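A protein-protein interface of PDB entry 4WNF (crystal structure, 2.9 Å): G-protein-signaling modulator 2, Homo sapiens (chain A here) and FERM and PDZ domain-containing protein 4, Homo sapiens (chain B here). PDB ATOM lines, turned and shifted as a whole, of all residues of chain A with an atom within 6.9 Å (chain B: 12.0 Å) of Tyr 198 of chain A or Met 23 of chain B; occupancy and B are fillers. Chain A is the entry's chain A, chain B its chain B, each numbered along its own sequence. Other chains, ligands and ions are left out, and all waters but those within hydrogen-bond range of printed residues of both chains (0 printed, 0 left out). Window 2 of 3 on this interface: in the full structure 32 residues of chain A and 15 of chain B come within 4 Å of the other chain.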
ATOM      1  N   HIS A 138      10.246  13.036 -15.136  1.00  0.00           N
ATOM      2  CA  HIS A 138       9.182  12.846 -14.168  1.00  0.00           C
ATOM      3  C   HIS A 138       9.666  13.351 -12.843  1.00  0.00           C
ATOM      4  O   HIS A 138       9.127  14.306 -12.302  1.00  0.00           O
ATOM      5  CB  HIS A 138       8.798  11.380 -14.046  1.00  0.00           C
ATOM      6  CG  HIS A 138       7.834  11.105 -12.935  1.00  0.00           C
ATOM      7  ND1 HIS A 138       6.472  11.278 -13.070  1.00  0.00           N
ATOM      8  CD2 HIS A 138       8.033  10.677 -11.671  1.00  0.00           C
ATOM      9  CE1 HIS A 138       5.872  10.965 -11.939  1.00  0.00           C
ATOM     10  NE2 HIS A 138       6.797  10.587 -11.075  1.00  0.00           N
ATOM     11  N   LYS A 142       8.264  16.445 -10.678  1.00  0.00           N
ATOM     12  CA  LYS A 142       7.682  16.032  -9.413  1.00  0.00           C
ATOM     13  C   LYS A 142       8.292  16.834  -8.272  1.00  0.00           C
ATOM     14  O   LYS A 142       7.592  17.211  -7.339  1.00  0.00           O
ATOM     15  CB  LYS A 142       7.926  14.547  -9.188  1.00  0.00           C
ATOM     16  CG  LYS A 142       7.126  13.940  -8.048  1.00  0.00           C
ATOM     17  CD  LYS A 142       7.910  12.838  -7.327  1.00  0.00           C
ATOM     18  CE  LYS A 142       7.950  11.519  -8.097  1.00  0.00           C
ATOM     19  NZ  LYS A 142       9.168  10.695  -7.813  1.00  0.00           N
ATOM     20  N   PRO A 147       3.757  17.535  -4.040  1.00  0.00           N
ATOM     21  CA  PRO A 147       2.919  16.922  -5.098  1.00  0.00           C
ATOM     22  C   PRO A 147       1.400  17.141  -4.957  1.00  0.00           C
ATOM     23  O   PRO A 147       0.896  17.387  -3.859  1.00  0.00           O
ATOM     24  CB  PRO A 147       3.268  15.419  -5.014  1.00  0.00           C
ATOM     25  CG  PRO A 147       4.217  15.258  -3.867  1.00  0.00           C
ATOM     26  CD  PRO A 147       4.211  16.529  -3.065  1.00  0.00           C
ATOM     27  N   PRO A 149      -2.677  18.646  -3.934  1.00  0.00           N
ATOM     28  CA  PRO A 149      -3.891  19.120  -4.602  1.00  0.00           C
ATOM     29  C   PRO A 149      -3.710  20.475  -5.288  1.00  0.00           C
ATOM     30  O   PRO A 149      -4.077  20.622  -6.458  1.00  0.00           O
ATOM     31  CB  PRO A 149      -4.910  19.222  -3.458  1.00  0.00           C
ATOM     32  CG  PRO A 149      -4.104  19.373  -2.212  1.00  0.00           C
ATOM     33  CD  PRO A 149      -2.727  18.825  -2.471  1.00  0.00           C
ATOM     34  N   VAL A 152      -1.822  20.342  -8.904  1.00  0.00           N
ATOM     35  CA  VAL A 152      -2.586  20.043 -10.138  1.00  0.00           C
ATOM     36  C   VAL A 152      -3.414  21.218 -10.701  1.00  0.00           C
ATOM     37  O   VAL A 152      -3.615  21.312 -11.915  1.00  0.00           O
ATOM     38  CB  VAL A 152      -3.528  18.840  -9.929  1.00  0.00           C
ATOM     39  N   ASN A 192       4.564   4.195 -14.254  1.00  0.00           N
ATOM     40  CA  ASN A 192       5.105   5.541 -14.185  1.00  0.00           C
ATOM     41  C   ASN A 192       4.360   6.461 -15.138  1.00  0.00           C
ATOM     42  O   ASN A 192       4.159   7.638 -14.851  1.00  0.00           O
ATOM     43  CB  ASN A 192       6.606   5.562 -14.480  1.00  0.00           C
ATOM     44  CG  ASN A 192       7.433   4.825 -13.431  1.00  0.00           C
ATOM     45  OD1 ASN A 192       6.920   4.334 -12.415  1.00  0.00           O
ATOM     46  ND2 ASN A 192       8.726   4.730 -13.691  1.00  0.00           N
ATOM     47  N   LEU A 193       3.914   5.936 -16.269  1.00  0.00           N
ATOM     48  CA  LEU A 193       3.179   6.785 -17.175  1.00  0.00           C
ATOM     49  C   LEU A 193       1.956   7.291 -16.445  1.00  0.00           C
ATOM     50  O   LEU A 193       1.607   8.453 -16.576  1.00  0.00           O
ATOM     51  CB  LEU A 193       2.789   6.059 -18.456  1.00  0.00           C
ATOM     52  CG  LEU A 193       1.947   6.887 -19.440  1.00  0.00           C
ATOM     53  CD1 LEU A 193       2.568   8.229 -19.741  1.00  0.00           C
ATOM     54  CD2 LEU A 193       1.720   6.152 -20.750  1.00  0.00           C
ATOM     55  N   GLY A 194       1.324   6.424 -15.659  1.00  0.00           N
ATOM     56  CA  GLY A 194       0.069   6.768 -14.989  1.00  0.00           C
ATOM     57  C   GLY A 194       0.206   7.821 -13.901  1.00  0.00           C
ATOM     58  O   GLY A 194      -0.590   8.764 -13.836  1.00  0.00           O
ATOM     59  N   ASN A 195       1.204   7.655 -13.033  1.00  0.00           N
ATOM     60  CA  ASN A 195       1.525   8.663 -12.018  1.00  0.00           C
ATOM     61  C   ASN A 195       1.858  10.026 -12.607  1.00  0.00           C
ATOM     62  O   ASN A 195       1.504  11.049 -12.035  1.00  0.00           O
ATOM     63  CB  ASN A 195       2.715   8.224 -11.199  1.00  0.00           C
ATOM     64  CG  ASN A 195       2.452   6.963 -10.426  1.00  0.00           C
ATOM     65  OD1 ASN A 195       1.379   6.796  -9.860  1.00  0.00           O
ATOM     66  ND2 ASN A 195       3.443   6.072 -10.373  1.00  0.00           N
ATOM     67  N   THR A 196       2.574  10.032 -13.728  1.00  0.00           N
ATOM     68  CA  THR A 196       2.886  11.265 -14.450  1.00  0.00           C
ATOM     69  C   THR A 196       1.580  11.950 -14.879  1.00  0.00           C
ATOM     70  O   THR A 196       1.430  13.168 -14.764  1.00  0.00           O
ATOM     71  CB  THR A 196       3.748  10.975 -15.700  1.00  0.00           C
ATOM     72  OG1 THR A 196       4.800  10.060 -15.366  1.00  0.00           O
ATOM     73  CG2 THR A 196       4.346  12.245 -16.269  1.00  0.00           C
ATOM     74  N   HIS A 197       0.629  11.159 -15.359  1.00  0.00           N
ATOM     75  CA  HIS A 197      -0.680  11.700 -15.714  1.00  0.00           C
ATOM     76  C   HIS A 197      -1.386  12.232 -14.471  1.00  0.00           C
ATOM     77  O   HIS A 197      -1.932  13.347 -14.465  1.00  0.00           O
ATOM     78  CB  HIS A 197      -1.550  10.638 -16.373  1.00  0.00           C
ATOM     79  CG  HIS A 197      -1.254  10.431 -17.819  1.00  0.00           C
ATOM     80  ND1 HIS A 197      -1.365  11.443 -18.751  1.00  0.00           N
ATOM     81  CD2 HIS A 197      -0.879   9.325 -18.503  1.00  0.00           C
ATOM     82  CE1 HIS A 197      -1.060  10.973 -19.948  1.00  0.00           C
ATOM     83  NE2 HIS A 197      -0.762   9.690 -19.824  1.00  0.00           N
ATOM     84  N   TYR A 198      -1.374  11.423 -13.424  1.00  0.00           N
ATOM     85  CA  TYR A 198      -1.953  11.827 -12.165  1.00  0.00           C
ATOM     86  C   TYR A 198      -1.538  13.273 -11.825  1.00  0.00           C
ATOM     87  O   TYR A 198      -2.398  14.140 -11.632  1.00  0.00           O
ATOM     88  CB  TYR A 198      -1.540  10.817 -11.095  1.00  0.00           C
ATOM     89  CG  TYR A 198      -1.826  11.200  -9.670  1.00  0.00           C
ATOM     90  CD1 TYR A 198      -3.085  11.620  -9.275  1.00  0.00           C
ATOM     91  CD2 TYR A 198      -0.839  11.093  -8.708  1.00  0.00           C
ATOM     92  CE1 TYR A 198      -3.344  11.953  -7.953  1.00  0.00           C
ATOM     93  CE2 TYR A 198      -1.079  11.423  -7.389  1.00  0.00           C
ATOM     94  CZ  TYR A 198      -2.331  11.851  -7.012  1.00  0.00           C
ATOM     95  OH  TYR A 198      -2.548  12.169  -5.693  1.00  0.00           O
ATOM     96  N   LEU A 199      -0.231  13.536 -11.815  1.00  0.00           N
ATOM     97  CA  LEU A 199       0.299  14.857 -11.469  1.00  0.00           C
ATOM     98  C   LEU A 199      -0.149  15.909 -12.459  1.00  0.00           C
ATOM     99  O   LEU A 199      -0.592  16.989 -12.071  1.00  0.00           O
ATOM    100  CB  LEU A 199       1.824  14.845 -11.442  1.00  0.00           C
ATOM    101  CG  LEU A 199       2.493  13.981 -10.380  1.00  0.00           C
ATOM    102  CD1 LEU A 199       4.001  13.931 -10.600  1.00  0.00           C
ATOM    103  CD2 LEU A 199       2.168  14.518  -8.999  1.00  0.00           C
ATOM    104  N   LEU A 200      -0.035  15.592 -13.741  1.00  0.00           N
ATOM    105  CA  LEU A 200      -0.487  16.505 -14.779  1.00  0.00           C
ATOM    106  C   LEU A 200      -1.972  16.859 -14.690  1.00  0.00           C
ATOM    107  O   LEU A 200      -2.408  17.806 -15.322  1.00  0.00           O
ATOM    108  CB  LEU A 200      -0.195  15.915 -16.155  1.00  0.00           C
ATOM    109  CG  LEU A 200       1.206  16.204 -16.682  1.00  0.00           C
ATOM    110  CD1 LEU A 200       1.534  15.253 -17.814  1.00  0.00           C
ATOM    111  CD2 LEU A 200       1.320  17.651 -17.144  1.00  0.00           C
ATOM    112  N   GLY A 201      -2.740  16.091 -13.922  1.00  0.00           N
ATOM    113  CA  GLY A 201      -4.165  16.322 -13.787  1.00  0.00           C
ATOM    114  C   GLY A 201      -4.988  15.529 -14.784  1.00  0.00           C
ATOM    115  O   GLY A 201      -6.168  15.799 -14.969  1.00  0.00           O
ATOM    116  N   ASN A 202      -4.371  14.550 -15.433  1.00  0.00           N
ATOM    117  CA  ASN A 202      -5.056  13.761 -16.440  1.00  0.00           C
ATOM    118  C   ASN A 202      -5.448  12.447 -15.784  1.00  0.00           C
ATOM    119  O   ASN A 202      -4.775  11.436 -15.932  1.00  0.00           O
ATOM    120  CB  ASN A 202      -4.151  13.543 -17.664  1.00  0.00           C
ATOM    121  CG  ASN A 202      -3.751  14.856 -18.360  1.00  0.00           C
ATOM    122  OD1 ASN A 202      -4.345  15.918 -18.146  1.00  0.00           O
ATOM    123  ND2 ASN A 202      -2.741  14.775 -19.214  1.00  0.00           N
ATOM    124  N   PHE A 203      -6.544  12.471 -15.042  1.00  0.00           N
ATOM    125  CA  PHE A 203      -6.864  11.371 -14.141  1.00  0.00           C
ATOM    126  C   PHE A 203      -7.535  10.187 -14.826  1.00  0.00           C
ATOM    127  O   PHE A 203      -7.242   9.036 -14.510  1.00  0.00           O
ATOM    128  CB  PHE A 203      -7.718  11.887 -12.998  1.00  0.00           C
ATOM    129  CG  PHE A 203      -7.073  13.004 -12.240  1.00  0.00           C
ATOM    130  CD1 PHE A 203      -5.938  12.771 -11.468  1.00  0.00           C
ATOM    131  CD2 PHE A 203      -7.574  14.293 -12.323  1.00  0.00           C
ATOM    132  CE1 PHE A 203      -5.332  13.804 -10.780  1.00  0.00           C
ATOM    133  CE2 PHE A 203      -6.972  15.330 -11.634  1.00  0.00           C
ATOM    134  CZ  PHE A 203      -5.849  15.084 -10.864  1.00  0.00           C
ATOM    135  N   ASP A 205      -6.953   9.454 -17.921  1.00  0.00           N
ATOM    136  CA  ASP A 205      -5.736   8.888 -18.525  1.00  0.00           C
ATOM    137  C   ASP A 205      -4.874   8.093 -17.539  1.00  0.00           C
ATOM    138  O   ASP A 205      -4.240   7.105 -17.897  1.00  0.00           O
ATOM    139  CB  ASP A 205      -4.896  10.001 -19.124  1.00  0.00           C
ATOM    140  CG  ASP A 205      -5.417  10.453 -20.451  1.00  0.00           C
ATOM    141  OD1 ASP A 205      -5.664   9.567 -21.290  1.00  0.00           O
ATOM    142  OD2 ASP A 205      -5.572  11.678 -20.659  1.00  0.00           O
ATOM    143  N   ALA A 206      -4.848   8.552 -16.299  1.00  0.00           N
ATOM    144  CA  ALA A 206      -4.144   7.870 -15.242  1.00  0.00           C
ATOM    145  C   ALA A 206      -4.662   6.457 -15.082  1.00  0.00           C
ATOM    146  O   ALA A 206      -3.889   5.503 -14.959  1.00  0.00           O
ATOM    147  CB  ALA A 206      -4.313   8.634 -13.946  1.00  0.00           C
ATOM    148  N   HIS A 210      -2.811   2.618 -15.365  1.00  0.00           N
ATOM    149  CA  HIS A 210      -2.660   1.677 -14.261  1.00  0.00           C
ATOM    150  C   HIS A 210      -3.444   0.382 -14.441  1.00  0.00           C
ATOM    151  O   HIS A 210      -3.016  -0.667 -13.971  1.00  0.00           O
ATOM    152  CB  HIS A 210      -3.005   2.335 -12.937  1.00  0.00           C
ATOM    153  CG  HIS A 210      -1.963   3.297 -12.470  1.00  0.00           C
ATOM    154  ND1 HIS A 210      -2.148   4.664 -12.507  1.00  0.00           N
ATOM    155  CD2 HIS A 210      -0.719   3.092 -11.973  1.00  0.00           C
ATOM    156  CE1 HIS A 210      -1.066   5.260 -12.042  1.00  0.00           C
ATOM    157  NE2 HIS A 210      -0.183   4.329 -11.717  1.00  0.00           N
ATOM    158  N   SER A 231      -3.261   0.706  -5.403  1.00  0.00           N
ATOM    159  CA  SER A 231      -2.946   1.918  -4.716  1.00  0.00           C
ATOM    160  C   SER A 231      -3.099   3.098  -5.666  1.00  0.00           C
ATOM    161  O   SER A 231      -3.943   3.978  -5.405  1.00  0.00           O
ATOM    162  CB  SER A 231      -1.549   1.868  -4.118  1.00  0.00           C
ATOM    163  OG  SER A 231      -1.239   3.119  -3.529  1.00  0.00           O
ATOM    164  N   ASN A 232      -2.336   3.108  -6.775  1.00  0.00           N
ATOM    165  CA  ASN A 232      -2.316   4.304  -7.624  1.00  0.00           C
ATOM    166  C   ASN A 232      -3.712   4.545  -8.196  1.00  0.00           C
ATOM    167  O   ASN A 232      -4.156   5.684  -8.281  1.00  0.00           O
ATOM    168  CB  ASN A 232      -1.217   4.279  -8.701  1.00  0.00           C
ATOM    169  CG  ASN A 232       0.192   4.266  -8.100  1.00  0.00           C
ATOM    170  OD1 ASN A 232       0.639   5.238  -7.488  1.00  0.00           O
ATOM    171  ND2 ASN A 232       0.899   3.166  -8.290  1.00  0.00           N
ATOM    172  N   ASN A 235      -5.997   6.510  -5.783  1.00  0.00           N
ATOM    173  CA  ASN A 235      -5.737   7.946  -5.747  1.00  0.00           C
ATOM    174  C   ASN A 235      -6.455   8.753  -6.831  1.00  0.00           C
ATOM    175  O   ASN A 235      -6.950   9.847  -6.568  1.00  0.00           O
ATOM    176  CB  ASN A 235      -4.232   8.211  -5.818  1.00  0.00           C
ATOM    177  CG  ASN A 235      -3.455   7.451  -4.756  1.00  0.00           C
ATOM    178  OD1 ASN A 235      -4.017   6.634  -4.013  1.00  0.00           O
ATOM    179  ND2 ASN A 235      -2.152   7.703  -4.692  1.00  0.00           N
ATOM    180  N   ALA A 236      -6.517   8.222  -8.045  1.00  0.00           N
ATOM    181  CA  ALA A 236      -7.064   8.981  -9.170  1.00  0.00           C
ATOM    182  C   ALA A 236      -8.567   9.166  -9.032  1.00  0.00           C
ATOM    183  O   ALA A 236      -9.102  10.256  -9.283  1.00  0.00           O
ATOM    184  CB  ALA A 236      -6.743   8.292 -10.485  1.00  0.00           C
ATOM    185  N   PHE A 239      -9.559  11.831  -6.955  1.00  0.00           N
ATOM    186  CA  PHE A 239      -9.523  13.125  -7.636  1.00  0.00           C
ATOM    187  C   PHE A 239     -10.672  13.339  -8.613  1.00  0.00           C
ATOM    188  O   PHE A 239     -11.004  14.479  -8.931  1.00  0.00           O
ATOM    189  CB  PHE A 239      -8.179  13.346  -8.325  1.00  0.00           C
ATOM    190  CG  PHE A 239      -7.134  13.921  -7.411  1.00  0.00           C
ATOM    191  CD1 PHE A 239      -6.653  13.184  -6.339  1.00  0.00           C
ATOM    192  CD2 PHE A 239      -6.645  15.215  -7.608  1.00  0.00           C
ATOM    193  CE1 PHE A 239      -5.696  13.718  -5.487  1.00  0.00           C
ATOM    194  CE2 PHE A 239      -5.687  15.754  -6.760  1.00  0.00           C
ATOM    195  CZ  PHE A 239      -5.211  15.004  -5.700  1.00  0.00           C
ATOM    196  N   HIS B  22       4.188   9.923  -1.825  1.00  0.00           N
ATOM    197  CA  HIS B  22       2.708   9.694  -1.872  1.00  0.00           C
ATOM    198  C   HIS B  22       2.353   8.555  -2.841  1.00  0.00           C
ATOM    199  O   HIS B  22       1.699   7.575  -2.462  1.00  0.00           O
ATOM    200  CB  HIS B  22       1.982  10.980  -2.299  1.00  0.00           C
ATOM    201  CG  HIS B  22       0.546  11.042  -1.867  1.00  0.00           C
ATOM    202  ND1 HIS B  22      -0.138  12.232  -1.738  1.00  0.00           N
ATOM    203  CD2 HIS B  22      -0.326  10.067  -1.513  1.00  0.00           C
ATOM    204  CE1 HIS B  22      -1.373  11.987  -1.335  1.00  0.00           C
ATOM    205  NE2 HIS B  22      -1.512  10.682  -1.190  1.00  0.00           N
ATOM    206  N   MET B  23       2.792   8.710  -4.093  1.00  0.00           N
ATOM    207  CA  MET B  23       2.536   7.734  -5.165  1.00  0.00           C
ATOM    208  C   MET B  23       3.616   6.665  -5.256  1.00  0.00           C
ATOM    209  O   MET B  23       4.768   6.857  -4.837  1.00  0.00           O
ATOM    210  CB  MET B  23       2.446   8.433  -6.514  1.00  0.00           C
ATOM    211  CG  MET B  23       3.795   8.917  -7.037  1.00  0.00           C
ATOM    212  SD  MET B  23       3.695  10.245  -8.251  1.00  0.00           S
ATOM    213  CE  MET B  23       2.334  11.199  -7.599  1.00  0.00           C
ATOM    214  N   GLU B  24       3.235   5.549  -5.857  1.00  0.00           N
ATOM    215  CA  GLU B  24       4.068   4.370  -5.871  1.00  0.00           C
ATOM    216  C   GLU B  24       4.593   4.200  -7.280  1.00  0.00           C
ATOM    217  O   GLU B  24       3.831   4.289  -8.247  1.00  0.00           O
ATOM    218  CB  GLU B  24       3.252   3.152  -5.438  1.00  0.00           C
ATOM    219  CG  GLU B  24       3.006   3.060  -3.928  1.00  0.00           C
ATOM    220  CD  GLU B  24       3.780   1.917  -3.285  1.00  0.00           C
ATOM    221  OE1 GLU B  24       5.029   1.873  -3.427  1.00  0.00           O
ATOM    222  OE2 GLU B  24       3.132   1.051  -2.654  1.00  0.00           O
ATOM    223  N   MET B  25       5.895   3.968  -7.391  1.00  0.00           N
ATOM    224  CA  MET B  25       6.578   4.036  -8.662  1.00  0.00           C
ATOM    225  C   MET B  25       7.230   2.713  -8.975  1.00  0.00           C
ATOM    226  O   MET B  25       7.416   1.869  -8.090  1.00  0.00           O
ATOM    227  CB  MET B  25       7.643   5.118  -8.615  1.00  0.00           C
ATOM    228  CG  MET B  25       7.093   6.483  -8.263  1.00  0.00           C
ATOM    229  SD  MET B  25       6.341   7.310  -9.671  1.00  0.00           S
ATOM    230  CE  MET B  25       7.831   7.737 -10.562  1.00  0.00           C
ATOM    231  N   GLU B  26       7.574   2.545 -10.249  1.00  0.00           N
ATOM    232  CA  GLU B  26       8.182   1.318 -10.724  1.00  0.00           C
ATOM    233  C   GLU B  26       9.695   1.416 -10.549  1.00  0.00           C
ATOM    234  O   GLU B  26      10.250   2.513 -10.565  1.00  0.00           O
ATOM    235  CB  GLU B  26       7.797   1.073 -12.189  1.00  0.00           C
ATOM    236  CG  GLU B  26       6.281   1.061 -12.474  1.00  0.00           C
ATOM    237  CD  GLU B  26       5.511  -0.075 -11.778  1.00  0.00           C
ATOM    238  OE1 GLU B  26       5.920  -1.251 -11.932  1.00  0.00           O
ATOM    239  OE2 GLU B  26       4.476   0.199 -11.098  1.00  0.00           O
ATOM    240  N   PRO B  27      10.370   0.273 -10.386  1.00  0.00           N
ATOM    241  CA  PRO B  27      11.817   0.310 -10.203  1.00  0.00           C
ATOM    242  C   PRO B  27      12.553   0.815 -11.435  1.00  0.00           C
ATOM    243  O   PRO B  27      11.974   0.904 -12.511  1.00  0.00           O
ATOM    244  CB  PRO B  27      12.170  -1.158  -9.973  1.00  0.00           C
ATOM    245  CG  PRO B  27      11.132  -1.910 -10.746  1.00  0.00           C
ATOM    246  CD  PRO B  27       9.875  -1.101 -10.593  1.00  0.00           C
ATOM    247  N   GLU B  28      13.830   1.136 -11.272  1.00  0.00           N
ATOM    248  CA  GLU B  28      14.662   1.531 -12.402  1.00  0.00           C
ATOM    249  C   GLU B  28      15.244   0.299 -13.060  1.00  0.00           C
ATOM    250  O   GLU B  28      15.409  -0.744 -12.433  1.00  0.00           O
ATOM    251  CB  GLU B  28      15.831   2.415 -11.963  1.00  0.00           C
ATOM    252  CG  GLU B  28      15.478   3.798 -11.437  1.00  0.00           C
ATOM    253  CD  GLU B  28      15.287   3.863  -9.918  1.00  0.00           C
ATOM    254  OE1 GLU B  28      14.716   4.873  -9.442  1.00  0.00           O
ATOM    255  OE2 GLU B  28      15.709   2.929  -9.194  1.00  0.00           O
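The side-chain amide nitrogen of Asn 195 of chain A sits at hydrogen-bond distance from the backbone carbonyl oxygen of Glu 24 of chain B (2.8 Å). OD1 of Asn 192 of chain A sits at hydrogen-bond distance from N of Glu 26 of chain B, at 2.9 Å. A ring nitrogen (NE2) of His 138 of chain A sits close to the side-chain sulfur of Met 25 of chain B, at 3.6 Å. The side-chain amide oxygen of Asn 232 of chain A is in hydrogen-bond range of the backbone NH of Glu 24 of chain B. The side-chain sulfur of Met 25 of chain B sits at hydrogen-bond distance from the side-chain amide nitrogen of Asn 195 of chain A.
OD1 of Asn 195 of chain A lies within hydrogen-bond range of NE2 of His 210 of chain A (3.5 Å). OD1 of Asn 195 of chain A sits close to OD1 of Asn 232 of chain A (2.9 Å). The side-chain hydroxyl (OG1) of Thr 196 of chain A is in hydrogen-bond range of the backbone carbonyl oxygen (O) of Asn 192 of chain A (2.6 Å). OG1 of Thr 196 of chain A is in hydrogen-bond range of ND1 of His 138 of chain A, at 3.1 Å.
Printed residues of chain B within 4 Å of His 138 of chain A: Met 25 (3.1 Å). No residue of chain B comes within 4 Å of Pro 147 of chain A. Pro 149 of chain A touches none of the printed residues of chain B. No residue of chain B comes within 4 Å of Val 152 of chain A. Of the printed residues of chain B, Asn 192 of chain A touches Met 25 and Glu 26. No residue of chain B comes within 4 Å of Gly 194 of chain A. Asn 195 of chain A touches just these residues of chain B: Met 23 (3.7 Å), Glu 24 (2.8 Å) and Met 25 (3.2 Å). No residue of chain B comes within 4 Å of Thr 196 of chain A. No residue of chain B comes within 4 Å of His 197 of chain A. Tyr 198 of chain A touches just one residue of chain B: Met 23. No residue of chain B comes within 4 Å of Gly 201 of chain A. Asn 202 of chain A touches none of the printed residues of chain B. His 210 of chain A touches none of the printed residues of chain B. Asn 232 of chain A touches just these residues of chain B: Met 23 and Glu 24. No residue of chain B comes within 4 Å of Asn 235 of chain A. No residue of chain B comes within 4 Å of Ala 236 of chain A. Met 23 of chain B touches four residues of chain A. Printed residues of chain A within 4 Å of Glu 24 of chain B: Asn 195 and Asn 232. Of the printed residues of chain A, Met 25 of chain B touches His 138 (3.1 Å), Asn 192 (3.8 Å) and Asn 195 (3.2 Å). Printed residues of chain A within 4 Å of Glu 26 of chain B: Asn 192 (2.9 Å). The nearest residue of chain B that does not touch Tyr 198 of chain A is His 22 of chain B (4.5 Å). The nearest printed residue of chain A that does not touch Met 25 of chain B is Lys 142 of chain A (4.3 Å).
Of the 25 printed residues of chain A, 6 touch a printed residue of chain B. Hydrophobic or aromatic side chains of chain A that line the printed part of chain B: His 138, Tyr 198 and Leu 199. Printed residues of chain B that touch a printed residue of chain A: Met 23, Glu 24, Met 25 and Glu 26. Hydrophobic or aromatic side chains of chain B within 4 Å of the printed part of chain A: Met 23 and Met 25. Among the printed residues, no Asp or Glu carboxylate lies within 4 Å of a Lys or Arg side-chain nitrogen of the other chain.
CA of Met 25 of chain B touches OD1 of Asn 192 of chain A (3.8 Å). Met 23 of chain B touches Asn 195 of chain A (SD to CB, 3.7 Å). CD2 of Tyr 198 of chain A touches CE of Met 23 of chain B, 3.4 Å away. Leu 199 of chain A touches Met 23 of chain B. Asn 232 of chain A touches Met 23 of chain B.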
